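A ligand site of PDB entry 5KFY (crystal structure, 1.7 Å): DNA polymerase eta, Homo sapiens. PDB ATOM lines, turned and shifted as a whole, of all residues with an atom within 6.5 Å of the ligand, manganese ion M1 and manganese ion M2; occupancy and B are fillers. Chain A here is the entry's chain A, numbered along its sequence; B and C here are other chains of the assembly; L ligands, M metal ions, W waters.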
ATOM      1  N   ASP A  16     -35.570   4.533 -27.579  1.00  0.00           N
ATOM      2  CA  ASP A  16     -34.205   4.061 -27.756  1.00  0.00           C
ATOM      3  C   ASP A  16     -33.231   5.228 -27.878  1.00  0.00           C
ATOM      4  O   ASP A  16     -33.409   6.106 -28.730  1.00  0.00           O
ATOM      5  CB  ASP A  16     -34.117   3.164 -28.998  1.00  0.00           C
ATOM      6  CG  ASP A  16     -32.734   2.597 -29.216  1.00  0.00           C
ATOM      7  OD1 ASP A  16     -31.903   3.283 -29.839  1.00  0.00           O
ATOM      8  OD2 ASP A  16     -32.482   1.449 -28.777  1.00  0.00           O
ATOM      9  N   MET A  17     -32.230   5.302 -27.011  1.00  0.00           N
ATOM     10  CA  MET A  17     -31.295   6.394 -27.063  1.00  0.00           C
ATOM     11  C   MET A  17     -30.441   6.448 -28.340  1.00  0.00           C
ATOM     12  O   MET A  17     -30.083   5.470 -28.809  1.00  0.00           O
ATOM     13  CB  MET A  17     -30.362   6.313 -25.868  1.00  0.00           C
ATOM     14  CG  MET A  17     -31.038   6.040 -24.579  1.00  0.00           C
ATOM     15  SD  MET A  17     -32.272   7.306 -24.152  1.00  0.00           S
ATOM     16  CE  MET A  17     -31.289   8.768 -24.087  1.00  0.00           C
ATOM     17  N   ASP A  18     -30.168   7.615 -28.869  1.00  0.00           N
ATOM     18  CA  ASP A  18     -29.281   7.777 -29.977  1.00  0.00           C
ATOM     19  C   ASP A  18     -27.831   7.592 -29.555  1.00  0.00           C
ATOM     20  O   ASP A  18     -27.451   8.072 -28.557  1.00  0.00           O
ATOM     21  CB  ASP A  18     -29.432   9.161 -30.587  1.00  0.00           C
ATOM     22  CG  ASP A  18     -30.862   9.419 -31.089  1.00  0.00           C
ATOM     23  OD1 ASP A  18     -31.550   8.506 -31.382  1.00  0.00           O
ATOM     24  OD2 ASP A  18     -31.217  10.556 -31.174  1.00  0.00           O
ATOM     25  N   CYS A  19     -27.131   6.783 -30.321  1.00  0.00           N
ATOM     26  CA  CYS A  19     -25.711   6.548 -30.149  1.00  0.00           C
ATOM     27  C   CYS A  19     -25.262   6.544 -28.669  1.00  0.00           C
ATOM     28  O   CYS A  19     -24.438   7.259 -28.303  1.00  0.00           O
ATOM     29  CB  CYS A  19     -24.816   7.276 -31.085  1.00  0.00           C
ATOM     30  SG  CYS A  19     -24.998   9.048 -31.048  1.00  0.00           S
ATOM     31  N   PHE A  20     -25.898   5.709 -27.879  1.00  0.00           N
ATOM     32  CA  PHE A  20     -25.981   5.958 -26.474  1.00  0.00           C
ATOM     33  C   PHE A  20     -24.627   6.120 -25.729  1.00  0.00           C
ATOM     34  O   PHE A  20     -24.428   7.103 -25.109  1.00  0.00           O
ATOM     35  CB  PHE A  20     -26.755   4.838 -25.799  1.00  0.00           C
ATOM     36  CG  PHE A  20     -26.946   5.024 -24.324  1.00  0.00           C
ATOM     37  CD1 PHE A  20     -27.373   6.182 -23.828  1.00  0.00           C
ATOM     38  CD2 PHE A  20     -26.753   3.994 -23.477  1.00  0.00           C
ATOM     39  CE1 PHE A  20     -27.610   6.333 -22.485  1.00  0.00           C
ATOM     40  CE2 PHE A  20     -26.919   4.146 -22.131  1.00  0.00           C
ATOM     41  CZ  PHE A  20     -27.364   5.338 -21.651  1.00  0.00           C
ATOM     42  N   PHE A  21     -23.702   5.202 -25.885  1.00  0.00           N
ATOM     43  CA  PHE A  21     -22.433   5.308 -25.181  1.00  0.00           C
ATOM     44  C   PHE A  21     -21.686   6.557 -25.623  1.00  0.00           C
ATOM     45  O   PHE A  21     -21.001   7.203 -24.817  1.00  0.00           O
ATOM     46  CB  PHE A  21     -21.546   4.073 -25.406  1.00  0.00           C
ATOM     47  CG  PHE A  21     -22.010   2.834 -24.692  1.00  0.00           C
ATOM     48  CD1 PHE A  21     -23.295   2.739 -24.165  1.00  0.00           C
ATOM     49  CD2 PHE A  21     -21.161   1.752 -24.538  1.00  0.00           C
ATOM     50  CE1 PHE A  21     -23.718   1.589 -23.518  1.00  0.00           C
ATOM     51  CE2 PHE A  21     -21.577   0.608 -23.887  1.00  0.00           C
ATOM     52  CZ  PHE A  21     -22.852   0.529 -23.375  1.00  0.00           C
ATOM     53  N   VAL A  22     -21.817   6.906 -26.896  1.00  0.00           N
ATOM     54  CA  VAL A  22     -21.200   8.123 -27.410  1.00  0.00           C
ATOM     55  C   VAL A  22     -21.772   9.346 -26.707  1.00  0.00           C
ATOM     56  O   VAL A  22     -21.026  10.238 -26.296  1.00  0.00           O
ATOM     57  CB  VAL A  22     -21.399   8.246 -28.935  1.00  0.00           C
ATOM     58  CG1 VAL A  22     -21.201   9.687 -29.391  1.00  0.00           C
ATOM     59  CG2 VAL A  22     -20.437   7.308 -29.666  1.00  0.00           C
ATOM     60  N   GLN A  41     -13.339  -0.140 -26.816  1.00  0.00           N
ATOM     61  CA  GLN A  41     -12.851  -0.867 -25.645  1.00  0.00           C
ATOM     62  C   GLN A  41     -11.533  -1.543 -25.981  1.00  0.00           C
ATOM     63  O   GLN A  41     -11.375  -2.130 -27.059  1.00  0.00           O
ATOM     64  CB  GLN A  41     -13.887  -1.874 -25.144  1.00  0.00           C
ATOM     65  CG  GLN A  41     -14.492  -2.784 -26.177  1.00  0.00           C
ATOM     66  CD  GLN A  41     -15.679  -3.564 -25.627  1.00  0.00           C
ATOM     67  OE1 GLN A  41     -16.140  -3.322 -24.509  1.00  0.00           O
ATOM     68  NE2 GLN A  41     -16.177  -4.510 -26.418  1.00  0.00           N
ATOM     69  N   ILE A  51     -17.636   0.111 -30.248  1.00  0.00           N
ATOM     70  CA  ILE A  51     -18.948  -0.391 -29.844  1.00  0.00           C
ATOM     71  C   ILE A  51     -20.054   0.667 -29.953  1.00  0.00           C
ATOM     72  O   ILE A  51     -21.227   0.346 -29.755  1.00  0.00           O
ATOM     73  CB  ILE A  51     -18.941  -0.930 -28.403  1.00  0.00           C
ATOM     74  CG1 ILE A  51     -18.428   0.119 -27.407  1.00  0.00           C
ATOM     75  CG2 ILE A  51     -18.099  -2.203 -28.306  1.00  0.00           C
ATOM     76  CD1 ILE A  51     -18.510  -0.334 -25.965  1.00  0.00           C
ATOM     77  N   ALA A  52     -19.699   1.911 -30.279  1.00  0.00           N
ATOM     78  CA  ALA A  52     -20.693   2.965 -30.489  1.00  0.00           C
ATOM     79  C   ALA A  52     -20.129   4.065 -31.378  1.00  0.00           C
ATOM     80  O   ALA A  52     -18.949   4.404 -31.274  1.00  0.00           O
ATOM     81  CB  ALA A  52     -21.175   3.536 -29.160  1.00  0.00           C
ATOM     82  N   VAL A  53     -20.959   4.622 -32.251  1.00  0.00           N
ATOM     83  CA  VAL A  53     -20.517   5.570 -33.272  1.00  0.00           C
ATOM     84  C   VAL A  53     -21.464   6.759 -33.414  1.00  0.00           C
ATOM     85  O   VAL A  53     -22.674   6.585 -33.576  1.00  0.00           O
ATOM     86  CB  VAL A  53     -20.402   4.874 -34.662  1.00  0.00           C
ATOM     87  CG1 VAL A  53     -19.872   5.845 -35.691  1.00  0.00           C
ATOM     88  CG2 VAL A  53     -19.507   3.659 -34.585  1.00  0.00           C
ATOM     89  N   TYR A  55     -23.325   9.943 -35.191  1.00  0.00           N
ATOM     90  CA  TYR A  55     -23.900  10.023 -36.530  1.00  0.00           C
ATOM     91  C   TYR A  55     -23.004  10.781 -37.506  1.00  0.00           C
ATOM     92  O   TYR A  55     -22.984  10.472 -38.691  1.00  0.00           O
ATOM     93  CB  TYR A  55     -25.308  10.633 -36.444  1.00  0.00           C
ATOM     94  CG  TYR A  55     -26.321   9.603 -36.014  1.00  0.00           C
ATOM     95  CD1 TYR A  55     -26.554   9.347 -34.664  1.00  0.00           C
ATOM     96  CD2 TYR A  55     -27.020   8.846 -36.946  1.00  0.00           C
ATOM     97  CE1 TYR A  55     -27.463   8.371 -34.262  1.00  0.00           C
ATOM     98  CE2 TYR A  55     -27.925   7.872 -36.554  1.00  0.00           C
ATOM     99  CZ  TYR A  55     -28.147   7.646 -35.216  1.00  0.00           C
ATOM    100  OH  TYR A  55     -29.057   6.681 -34.825  1.00  0.00           O
ATOM    101  N   ARG A  58     -20.698   8.137 -38.641  1.00  0.00           N
ATOM    102  CA  ARG A  58     -21.366   7.145 -39.492  1.00  0.00           C
ATOM    103  C   ARG A  58     -21.359   7.578 -40.953  1.00  0.00           C
ATOM    104  O   ARG A  58     -21.378   6.739 -41.856  1.00  0.00           O
ATOM    105  CB  ARG A  58     -22.802   6.907 -39.019  1.00  0.00           C
ATOM    106  CG  ARG A  58     -22.891   6.380 -37.604  1.00  0.00           C
ATOM    107  CD  ARG A  58     -24.303   5.978 -37.223  1.00  0.00           C
ATOM    108  NE  ARG A  58     -24.384   5.686 -35.789  1.00  0.00           N
ATOM    109  CZ  ARG A  58     -25.436   5.164 -35.175  1.00  0.00           C
ATOM    110  NH1 ARG A  58     -26.520   4.845 -35.862  1.00  0.00           N
ATOM    111  NH2 ARG A  58     -25.399   4.954 -33.872  1.00  0.00           N
ATOM    112  N   ARG A  64     -20.018   0.013 -35.793  1.00  0.00           N
ATOM    113  CA  ARG A  64     -19.764  -0.893 -34.681  1.00  0.00           C
ATOM    114  C   ARG A  64     -19.004  -2.127 -35.186  1.00  0.00           C
ATOM    115  O   ARG A  64     -19.113  -2.477 -36.365  1.00  0.00           O
ATOM    116  CB  ARG A  64     -21.096  -1.292 -34.021  1.00  0.00           C
ATOM    117  CG  ARG A  64     -21.028  -2.446 -33.042  1.00  0.00           C
ATOM    118  CD  ARG A  64     -22.348  -2.609 -32.305  1.00  0.00           C
ATOM    119  NE  ARG A  64     -22.651  -1.425 -31.514  1.00  0.00           N
ATOM    120  CZ  ARG A  64     -23.798  -0.749 -31.579  1.00  0.00           C
ATOM    121  NH1 ARG A  64     -24.759  -1.146 -32.397  1.00  0.00           N
ATOM    122  NH2 ARG A  64     -23.970   0.322 -30.818  1.00  0.00           N
ATOM    123  N   LEU A  92     -18.424  -1.485 -17.630  1.00  0.00           N
ATOM    124  CA  LEU A  92     -19.504  -0.717 -18.258  1.00  0.00           C
ATOM    125  C   LEU A  92     -20.380   0.038 -17.263  1.00  0.00           C
ATOM    126  O   LEU A  92     -21.484   0.463 -17.605  1.00  0.00           O
ATOM    127  CB  LEU A  92     -20.378  -1.653 -19.093  1.00  0.00           C
ATOM    128  CG  LEU A  92     -19.658  -2.527 -20.120  1.00  0.00           C
ATOM    129  CD1 LEU A  92     -20.628  -3.482 -20.780  1.00  0.00           C
ATOM    130  CD2 LEU A  92     -18.982  -1.653 -21.157  1.00  0.00           C
ATOM    131  N   SER A 116     -33.033  -3.282 -23.216  1.00  0.00           N
ATOM    132  CA  SER A 116     -31.588  -3.273 -23.334  1.00  0.00           C
ATOM    133  C   SER A 116     -31.034  -2.159 -22.465  1.00  0.00           C
ATOM    134  O   SER A 116     -31.782  -1.467 -21.788  1.00  0.00           O
ATOM    135  CB  SER A 116     -31.138  -3.068 -24.773  1.00  0.00           C
ATOM    136  OG  SER A 116     -31.234  -1.707 -25.143  1.00  0.00           O
ATOM    137  N   ILE A 117     -29.714  -1.975 -22.507  1.00  0.00           N
ATOM    138  CA  ILE A 117     -29.100  -0.923 -21.719  1.00  0.00           C
ATOM    139  C   ILE A 117     -29.565   0.470 -22.172  1.00  0.00           C
ATOM    140  O   ILE A 117     -29.473   1.432 -21.406  1.00  0.00           O
ATOM    141  CB  ILE A 117     -27.552  -1.005 -21.787  1.00  0.00           C
ATOM    142  CG1 ILE A 117     -26.912  -0.220 -20.642  1.00  0.00           C
ATOM    143  CG2 ILE A 117     -27.050  -0.518 -23.133  1.00  0.00           C
ATOM    144  CD1 ILE A 117     -25.401  -0.405 -20.541  1.00  0.00           C
ATOM    145  N   ASP A 118     -30.096   0.595 -23.391  1.00  0.00           N
ATOM    146  CA  ASP A 118     -30.467   1.926 -23.862  1.00  0.00           C
ATOM    147  C   ASP A 118     -31.894   2.026 -24.410  1.00  0.00           C
ATOM    148  O   ASP A 118     -32.224   2.992 -25.099  1.00  0.00           O
ATOM    149  CB  ASP A 118     -29.480   2.432 -24.921  1.00  0.00           C
ATOM    150  CG  ASP A 118     -29.858   2.036 -26.347  1.00  0.00           C
ATOM    151  OD1 ASP A 118     -30.269   0.872 -26.582  1.00  0.00           O
ATOM    152  OD2 ASP A 118     -29.758   2.892 -27.240  1.00  0.00           O
ATOM    153  N   GLU A 119     -32.742   1.050 -24.102  1.00  0.00           N
ATOM    154  CA  GLU A 119     -34.115   1.151 -24.600  1.00  0.00           C
ATOM    155  C   GLU A 119     -35.133   0.449 -23.712  1.00  0.00           C
ATOM    156  O   GLU A 119     -34.805  -0.482 -22.974  1.00  0.00           O
ATOM    157  CB  GLU A 119     -34.214   0.594 -26.021  1.00  0.00           C
ATOM    158  CG  GLU A 119     -34.165  -0.914 -26.130  1.00  0.00           C
ATOM    159  CD  GLU A 119     -33.607  -1.368 -27.458  1.00  0.00           C
ATOM    160  OE1 GLU A 119     -34.397  -1.674 -28.367  1.00  0.00           O
ATOM    161  OE2 GLU A 119     -32.370  -1.362 -27.593  1.00  0.00           O
ATOM    162  N   SER A 216     -34.678   8.450 -29.867  1.00  0.00           N
ATOM    163  CA  SER A 216     -35.721   8.283 -30.862  1.00  0.00           C
ATOM    164  C   SER A 216     -36.802   7.386 -30.275  1.00  0.00           C
ATOM    165  O   SER A 216     -36.605   6.791 -29.211  1.00  0.00           O
ATOM    166  CB  SER A 216     -35.156   7.681 -32.141  1.00  0.00           C
ATOM    167  OG  SER A 216     -34.154   8.518 -32.686  1.00  0.00           O
ATOM    168  N   LYS A 227     -40.757  -1.085 -32.264  1.00  0.00           N
ATOM    169  CA  LYS A 227     -39.312  -1.192 -32.457  1.00  0.00           C
ATOM    170  C   LYS A 227     -38.924  -0.830 -33.892  1.00  0.00           C
ATOM    171  O   LYS A 227     -37.967  -0.100 -34.137  1.00  0.00           O
ATOM    172  CB  LYS A 227     -38.808  -2.593 -32.121  1.00  0.00           C
ATOM    173  CG  LYS A 227     -37.336  -2.823 -32.399  1.00  0.00           C
ATOM    174  CD  LYS A 227     -36.472  -2.081 -31.384  1.00  0.00           C
ATOM    175  CE  LYS A 227     -34.999  -2.344 -31.643  1.00  0.00           C
ATOM    176  NZ  LYS A 227     -34.127  -1.482 -30.798  1.00  0.00           N
ATOM    177  N   LYS A 234     -34.541   7.830 -37.014  1.00  0.00           N
ATOM    178  CA  LYS A 234     -33.470   8.227 -36.093  1.00  0.00           C
ATOM    179  C   LYS A 234     -32.390   9.057 -36.816  1.00  0.00           C
ATOM    180  O   LYS A 234     -32.207   8.897 -38.018  1.00  0.00           O
ATOM    181  CB  LYS A 234     -32.840   6.979 -35.453  1.00  0.00           C
ATOM    182  CG  LYS A 234     -32.268   5.981 -36.451  1.00  0.00           C
ATOM    183  CD  LYS A 234     -31.611   4.804 -35.741  1.00  0.00           C
ATOM    184  CE  LYS A 234     -30.760   3.977 -36.693  1.00  0.00           C
ATOM    185  NZ  LYS A 234     -30.137   2.808 -36.010  1.00  0.00           N
ATOM    186  N   PRO A 235     -31.670   9.924 -36.082  1.00  0.00           N
ATOM    187  CA  PRO A 235     -31.800  10.147 -34.638  1.00  0.00           C
ATOM    188  C   PRO A 235     -32.709  11.320 -34.275  1.00  0.00           C
ATOM    189  O   PRO A 235     -33.109  12.083 -35.156  1.00  0.00           O
ATOM    190  CB  PRO A 235     -30.362  10.463 -34.223  1.00  0.00           C
ATOM    191  CG  PRO A 235     -29.839  11.251 -35.386  1.00  0.00           C
ATOM    192  CD  PRO A 235     -30.536  10.692 -36.627  1.00  0.00           C
ATOM    193  P    DT B   8     -31.200  -5.627 -31.871  1.00  0.00           P
ATOM    194  OP1  DT B   8     -32.166  -4.601 -32.311  1.00  0.00           O
ATOM    195  OP2  DT B   8     -30.055  -5.966 -32.743  1.00  0.00           O
ATOM    196  O5'  DT B   8     -30.579  -5.231 -30.434  1.00  0.00           O
ATOM    197  C5'  DT B   8     -31.300  -4.448 -29.422  1.00  0.00           C
ATOM    198  C4'  DT B   8     -30.289  -3.936 -28.401  1.00  0.00           C
ATOM    199  O4'  DT B   8     -29.402  -5.064 -28.178  1.00  0.00           O
ATOM    200  C3'  DT B   8     -29.443  -2.809 -28.993  1.00  0.00           C
ATOM    201  O3'  DT B   8     -29.400  -1.718 -28.096  1.00  0.00           O
ATOM    202  C2'  DT B   8     -28.060  -3.446 -29.187  1.00  0.00           C
ATOM    203  C1'  DT B   8     -28.079  -4.600 -28.208  1.00  0.00           C
ATOM    204  N1   DT B   8     -27.172  -5.717 -28.597  1.00  0.00           N
ATOM    205  C2   DT B   8     -26.121  -6.053 -27.769  1.00  0.00           C
ATOM    206  O2   DT B   8     -25.905  -5.490 -26.717  1.00  0.00           O
ATOM    207  N3   DT B   8     -25.342  -7.074 -28.220  1.00  0.00           N
ATOM    208  C4   DT B   8     -25.492  -7.791 -29.398  1.00  0.00           C
ATOM    209  O4   DT B   8     -24.726  -8.694 -29.713  1.00  0.00           O
ATOM    210  C5   DT B   8     -26.603  -7.386 -30.224  1.00  0.00           C
ATOM    211  C7   DT B   8     -26.856  -8.090 -31.532  1.00  0.00           C
ATOM    212  C6   DT B   8     -27.375  -6.375 -29.793  1.00  0.00           C
ATOM    213  P    DT C   3     -12.167 -10.984 -35.485  1.00  0.00           P
ATOM    214  OP1  DT C   3     -12.472 -12.418 -35.640  1.00  0.00           O
ATOM    215  OP2  DT C   3     -11.701 -10.185 -36.642  1.00  0.00           O
ATOM    216  O5'  DT C   3     -13.458 -10.246 -34.887  1.00  0.00           O
ATOM    217  C5'  DT C   3     -13.335  -8.973 -34.284  1.00  0.00           C
ATOM    218  C4'  DT C   3     -14.550  -8.652 -33.439  1.00  0.00           C
ATOM    219  O4'  DT C   3     -15.643  -8.295 -34.321  1.00  0.00           O
ATOM    220  C3'  DT C   3     -15.045  -9.809 -32.581  1.00  0.00           C
ATOM    221  O3'  DT C   3     -14.996  -9.444 -31.193  1.00  0.00           O
ATOM    222  C2'  DT C   3     -16.485 -10.076 -33.057  1.00  0.00           C
ATOM    223  C1'  DT C   3     -16.848  -8.795 -33.793  1.00  0.00           C
ATOM    224  N1   DT C   3     -17.802  -9.001 -34.918  1.00  0.00           N
ATOM    225  C2   DT C   3     -19.026  -8.386 -34.895  1.00  0.00           C
ATOM    226  O2   DT C   3     -19.396  -7.671 -33.974  1.00  0.00           O
ATOM    227  N3   DT C   3     -19.818  -8.643 -35.979  1.00  0.00           N
ATOM    228  C4   DT C   3     -19.508  -9.436 -37.068  1.00  0.00           C
ATOM    229  O4   DT C   3     -20.295  -9.607 -37.999  1.00  0.00           O
ATOM    230  C5   DT C   3     -18.199 -10.054 -37.036  1.00  0.00           C
ATOM    231  C7   DT C   3     -17.748 -10.929 -38.167  1.00  0.00           C
ATOM    232  C6   DT C   3     -17.412  -9.806 -35.979  1.00  0.00           C
ATOM    233  P    DT C   4     -14.059 -10.283 -30.183  1.00  0.00           P
ATOM    234  OP1  DT C   4     -12.657 -10.068 -30.597  1.00  0.00           O
ATOM    235  OP2  DT C   4     -14.617 -11.650 -30.105  1.00  0.00           O
ATOM    236  O5'  DT C   4     -14.304  -9.598 -28.760  1.00  0.00           O
ATOM    237  C5'  DT C   4     -13.433  -8.574 -28.264  1.00  0.00           C
ATOM    238  C4'  DT C   4     -14.086  -7.848 -27.101  1.00  0.00           C
ATOM    239  O4'  DT C   4     -15.329  -7.273 -27.561  1.00  0.00           O
ATOM    240  C3'  DT C   4     -14.447  -8.754 -25.919  1.00  0.00           C
ATOM    241  O3'  DT C   4     -14.315  -8.020 -24.714  1.00  0.00           O
ATOM    242  C2'  DT C   4     -15.913  -9.086 -26.203  1.00  0.00           C
ATOM    243  C1'  DT C   4     -16.395  -7.769 -26.779  1.00  0.00           C
ATOM    244  N1   DT C   4     -17.590  -7.869 -27.648  1.00  0.00           N
ATOM    245  C2   DT C   4     -18.552  -6.891 -27.558  1.00  0.00           C
ATOM    246  O2   DT C   4     -18.483  -5.967 -26.776  1.00  0.00           O
ATOM    247  N3   DT C   4     -19.607  -7.050 -28.410  1.00  0.00           N
ATOM    248  C4   DT C   4     -19.791  -8.051 -29.343  1.00  0.00           C
ATOM    249  O4   DT C   4     -20.786  -8.102 -30.067  1.00  0.00           O
ATOM    250  C5   DT C   4     -18.742  -9.044 -29.390  1.00  0.00           C
ATOM    251  C7   DT C   4     -18.835 -10.188 -30.367  1.00  0.00           C
ATOM    252  C6   DT C   4     -17.703  -8.902 -28.560  1.00  0.00           C
ATOM    253  P    DA C   5     -14.612  -8.718 -23.296  1.00  0.00           P
ATOM    254  OP1  DA C   5     -13.642  -8.171 -22.325  1.00  0.00           O
ATOM    255  OP2  DA C   5     -14.724 -10.177 -23.514  1.00  0.00           O
ATOM    256  O5'  DA C   5     -16.062  -8.173 -22.901  1.00  0.00           O
ATOM    257  C5'  DA C   5     -16.247  -6.783 -22.653  1.00  0.00           C
ATOM    258  C4'  DA C   5     -17.652  -6.509 -22.153  1.00  0.00           C
ATOM    259  O4'  DA C   5     -18.593  -6.626 -23.257  1.00  0.00           O
ATOM    260  C3'  DA C   5     -18.155  -7.463 -21.074  1.00  0.00           C
ATOM    261  O3'  DA C   5     -18.933  -6.761 -20.138  1.00  0.00           O
ATOM    262  C2'  DA C   5     -19.009  -8.451 -21.872  1.00  0.00           C
ATOM    263  C1'  DA C   5     -19.627  -7.512 -22.895  1.00  0.00           C
ATOM    264  N9   DA C   5     -20.084  -8.191 -24.099  1.00  0.00           N
ATOM    265  C8   DA C   5     -19.490  -9.267 -24.712  1.00  0.00           C
ATOM    266  N7   DA C   5     -20.112  -9.662 -25.786  1.00  0.00           N
ATOM    267  C5   DA C   5     -21.191  -8.796 -25.888  1.00  0.00           C
ATOM    268  C6   DA C   5     -22.240  -8.693 -26.821  1.00  0.00           C
ATOM    269  N6   DA C   5     -22.370  -9.516 -27.868  1.00  0.00           N
ATOM    270  N1   DA C   5     -23.153  -7.723 -26.639  1.00  0.00           N
ATOM    271  C2   DA C   5     -23.022  -6.909 -25.581  1.00  0.00           C
ATOM    272  N3   DA C   5     -22.077  -6.897 -24.639  1.00  0.00           N
ATOM    273  C4   DA C   5     -21.183  -7.887 -24.856  1.00  0.00           C
HETATM  274  P1  LIG L   1     -28.442   4.069 -32.442  1.00  0.00           P
HETATM  275  O1  LIG L   1     -29.477   3.385 -31.595  1.00  0.00           O
HETATM  276  O2  LIG L   1     -28.729   5.558 -32.504  1.00  0.00           O
HETATM  277  O3  LIG L   1     -28.428   3.485 -33.844  1.00  0.00           O
HETATM  278  P2  LIG L   1     -26.740   3.016 -30.482  1.00  0.00           P
HETATM  279  O4  LIG L   1     -27.592   3.559 -29.336  1.00  0.00           O
HETATM  280  O5  LIG L   1     -25.264   3.165 -30.154  1.00  0.00           O
HETATM  281  O6  LIG L   1     -27.002   3.858 -31.813  1.00  0.00           O
HETATM  282  P3  LIG L   1     -27.832   0.472 -29.932  1.00  0.00           P
HETATM  283  O7  LIG L   1     -29.175   1.020 -29.527  1.00  0.00           O
HETATM  284  O8  LIG L   1     -27.995  -0.751 -30.810  1.00  0.00           O
HETATM  285  O9  LIG L   1     -27.037   1.501 -30.815  1.00  0.00           O
HETATM  286  O10 LIG L   1     -26.994   0.079 -28.654  1.00  0.00           O
HETATM  287  C1  LIG L   1     -26.966   0.952 -27.561  1.00  0.00           C
HETATM  288  C2  LIG L   1     -25.644   0.866 -26.825  1.00  0.00           C
HETATM  289  O11 LIG L   1     -25.422  -0.478 -26.445  1.00  0.00           O
HETATM  290  C3  LIG L   1     -24.549   1.253 -27.689  1.00  0.00           C
HETATM  291  O12 LIG L   1     -24.258   2.638 -27.538  1.00  0.00           O
HETATM  292  C4  LIG L   1     -23.400   0.434 -27.305  1.00  0.00           C
HETATM  293  C5  LIG L   1     -24.040  -0.773 -26.722  1.00  0.00           C
HETATM  294  N1  LIG L   1     -23.968  -1.848 -27.637  1.00  0.00           N
HETATM  295  C6  LIG L   1     -24.794  -2.096 -28.680  1.00  0.00           C
HETATM  296  N2  LIG L   1     -24.426  -3.187 -29.309  1.00  0.00           N
HETATM  297  C7  LIG L   1     -23.338  -3.691 -28.703  1.00  0.00           C
HETATM  298  C8  LIG L   1     -22.524  -4.800 -28.912  1.00  0.00           C
HETATM  299  N3  LIG L   1     -22.804  -5.689 -30.001  1.00  0.00           N
HETATM  300  N4  LIG L   1     -21.495  -5.029 -28.100  1.00  0.00           N
HETATM  301  C9  LIG L   1     -21.203  -4.217 -27.062  1.00  0.00           C
HETATM  302  N5  LIG L   1     -21.984  -3.116 -26.826  1.00  0.00           N
HETATM  303  C10 LIG L   1     -23.031  -2.846 -27.618  1.00  0.00           C
HETATM  304 MN    MN M   1     -30.951   0.010 -28.487  1.00  0.00          MN
HETATM  305 MN    MN M   2     -29.754   3.256 -29.373  1.00  0.00          MN
HETATM  306  O   HOH W   1     -23.489   3.380 -32.249  1.00  0.00           O
HETATM  307  O   HOH W   2     -27.894  -1.973 -26.180  1.00  0.00           O
HETATM  308  O   HOH W   3     -25.027  -4.576 -31.982  1.00  0.00           O
HETATM  309  O   HOH W   4     -31.308  -0.637 -30.589  1.00  0.00           O
HETATM  310  O   HOH W   5     -30.810   1.245 -32.627  1.00  0.00           O
HETATM  311  O   HOH W   6     -26.821   1.398 -34.581  1.00  0.00           O
HETATM  312  O   HOH W   7     -21.432  -2.729 -24.074  1.00  0.00           O
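Of the 27 residues printed, 3 come within 4 Å of manganese ion M2.
The nearest printed residue that does not touch manganese ion M2 is Asp 18 (4.4 Å).
N1 of DA 5 of chain C lies close to a nitrogen (N4) of the ligand, 3.5 Å away.
Merely in contact with the ligand: Ile 51 (3.3 Å), Asp 18 (3.4 Å), Ala 52 (3.6 Å) and Ile 117 (3.7 Å).
Hydrophobic or aromatic side chains that line the ligand: Phe 20, Phe 21, Ile 51, Ala 52, Tyr 55 and Ile 117.
Within 4 Å of the ligand: Asp 16, Met 17, Asp 18, Cys 19, Phe 20, Phe 21, Ile 51, Ala 52, Tyr 55, Arg 58, Arg 64, Ile 117, Asp 118, Lys 234, DT 8 of chain B, DT 4 of chain C and DA 5 of chain C.
NH2 of Arg 64 lies within salt-bridge range of O5 of the ligand.
NH1 of Arg 58 is in salt-bridge range of O3 of the ligand (3.1 Å).
A nitrogen (N3) of the ligand sits at hydrogen-bond distance from O4 of DT 4 of chain C, 3.1 Å away.
The backbone NH (N) of Phe 20 lies within hydrogen-bond range of an oxygen (O5) of the ligand, at 3.5 Å.
NZ of Lys 234 is in salt-bridge range of O3 of the ligand, 2.8 Å away.
N3 of DT 8 of chain B lies within hydrogen-bond range of a nitrogen (N3) of the ligand (3.4 Å).
O2 of the ligand lies within hydrogen-bond range of OH of Tyr 55 (2.6 Å).
N of Phe 21 sits at hydrogen-bond distance from O12 of the ligand, 3.1 Å away.
N of Cys 19 is in hydrogen-bond range of O2 of the ligand.
The backbone NH of Asp 118 sits close to the side-chain hydroxyl of Ser 116, at 3.1 Å.
The backbone carbonyl oxygen of Asp 16 is in hydrogen-bond range of the backbone NH of Ser 216, 2.9 Å away.
The side-chain carboxylate of Asp 18 sits at hydrogen-bond distance from the side-chain hydroxyl of Ser 216, at 2.9 Å.
The side-chain hydroxyl (OG) of Ser 116 lies close to the backbone NH (N) of Glu 119, 3.3 Å away.
O of Val 53 sits at hydrogen-bond distance from NE of Arg 58.
OP1 of DT 8 of chain B lies within salt-bridge range of the side-chain amino group (NZ) of Lys 227 (3.98 Å).
O3' of DT 8 of chain B lies close to the side-chain hydroxyl (OG) of Ser 116 (3.5 Å).
The side-chain amino group of Lys 227 sits close to the side-chain carboxylate of Asp 16 (3.9 Å).
Manganese ion M2 is bound by OD2 of Asp 118 (2.2 Å).
Manganese ion M2 is bound by O4 of the ligand (2.2 Å).
OD1 of Asp 16 binds manganese ion M2.
Manganese ion M2 is bound by an oxygen (O1) of the ligand (2.2 Å).
Manganese ion M2 is bound by O of Met 17 (2.3 Å).
O7 of the ligand binds manganese ion M2.
Merely in contact with manganese ion M1: Ser 116.
Within 4 Å of manganese ion M1: Asp 16, Ser 116, Asp 118, Glu 119 and DT 8 of chain B.
The nearest printed residue that does not touch manganese ion M1 is Lys 227 (4.2 Å).
Manganese ion M1 is bound by OD2 of Asp 16.
Manganese ion M1 is bound by the side-chain carboxylate (OE2) of Glu 119 (2.2 Å).
OD1 of Asp 118 binds manganese ion M1, at 2.2 Å.
Manganese ion M1 is bound by water W4 (2.2 Å).
Manganese ion M1 is bound by an oxygen (O7) of the ligand (2.3 Å).
O3' of DT 8 of chain B is bound to manganese ion M1 (2.4 Å).
Water W4 lies within hydrogen-bond range of NZ of Lys 227 and O8 of the ligand.
Water W3 lies within hydrogen-bond range of N2 of the ligand and NH1 of Arg 64.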
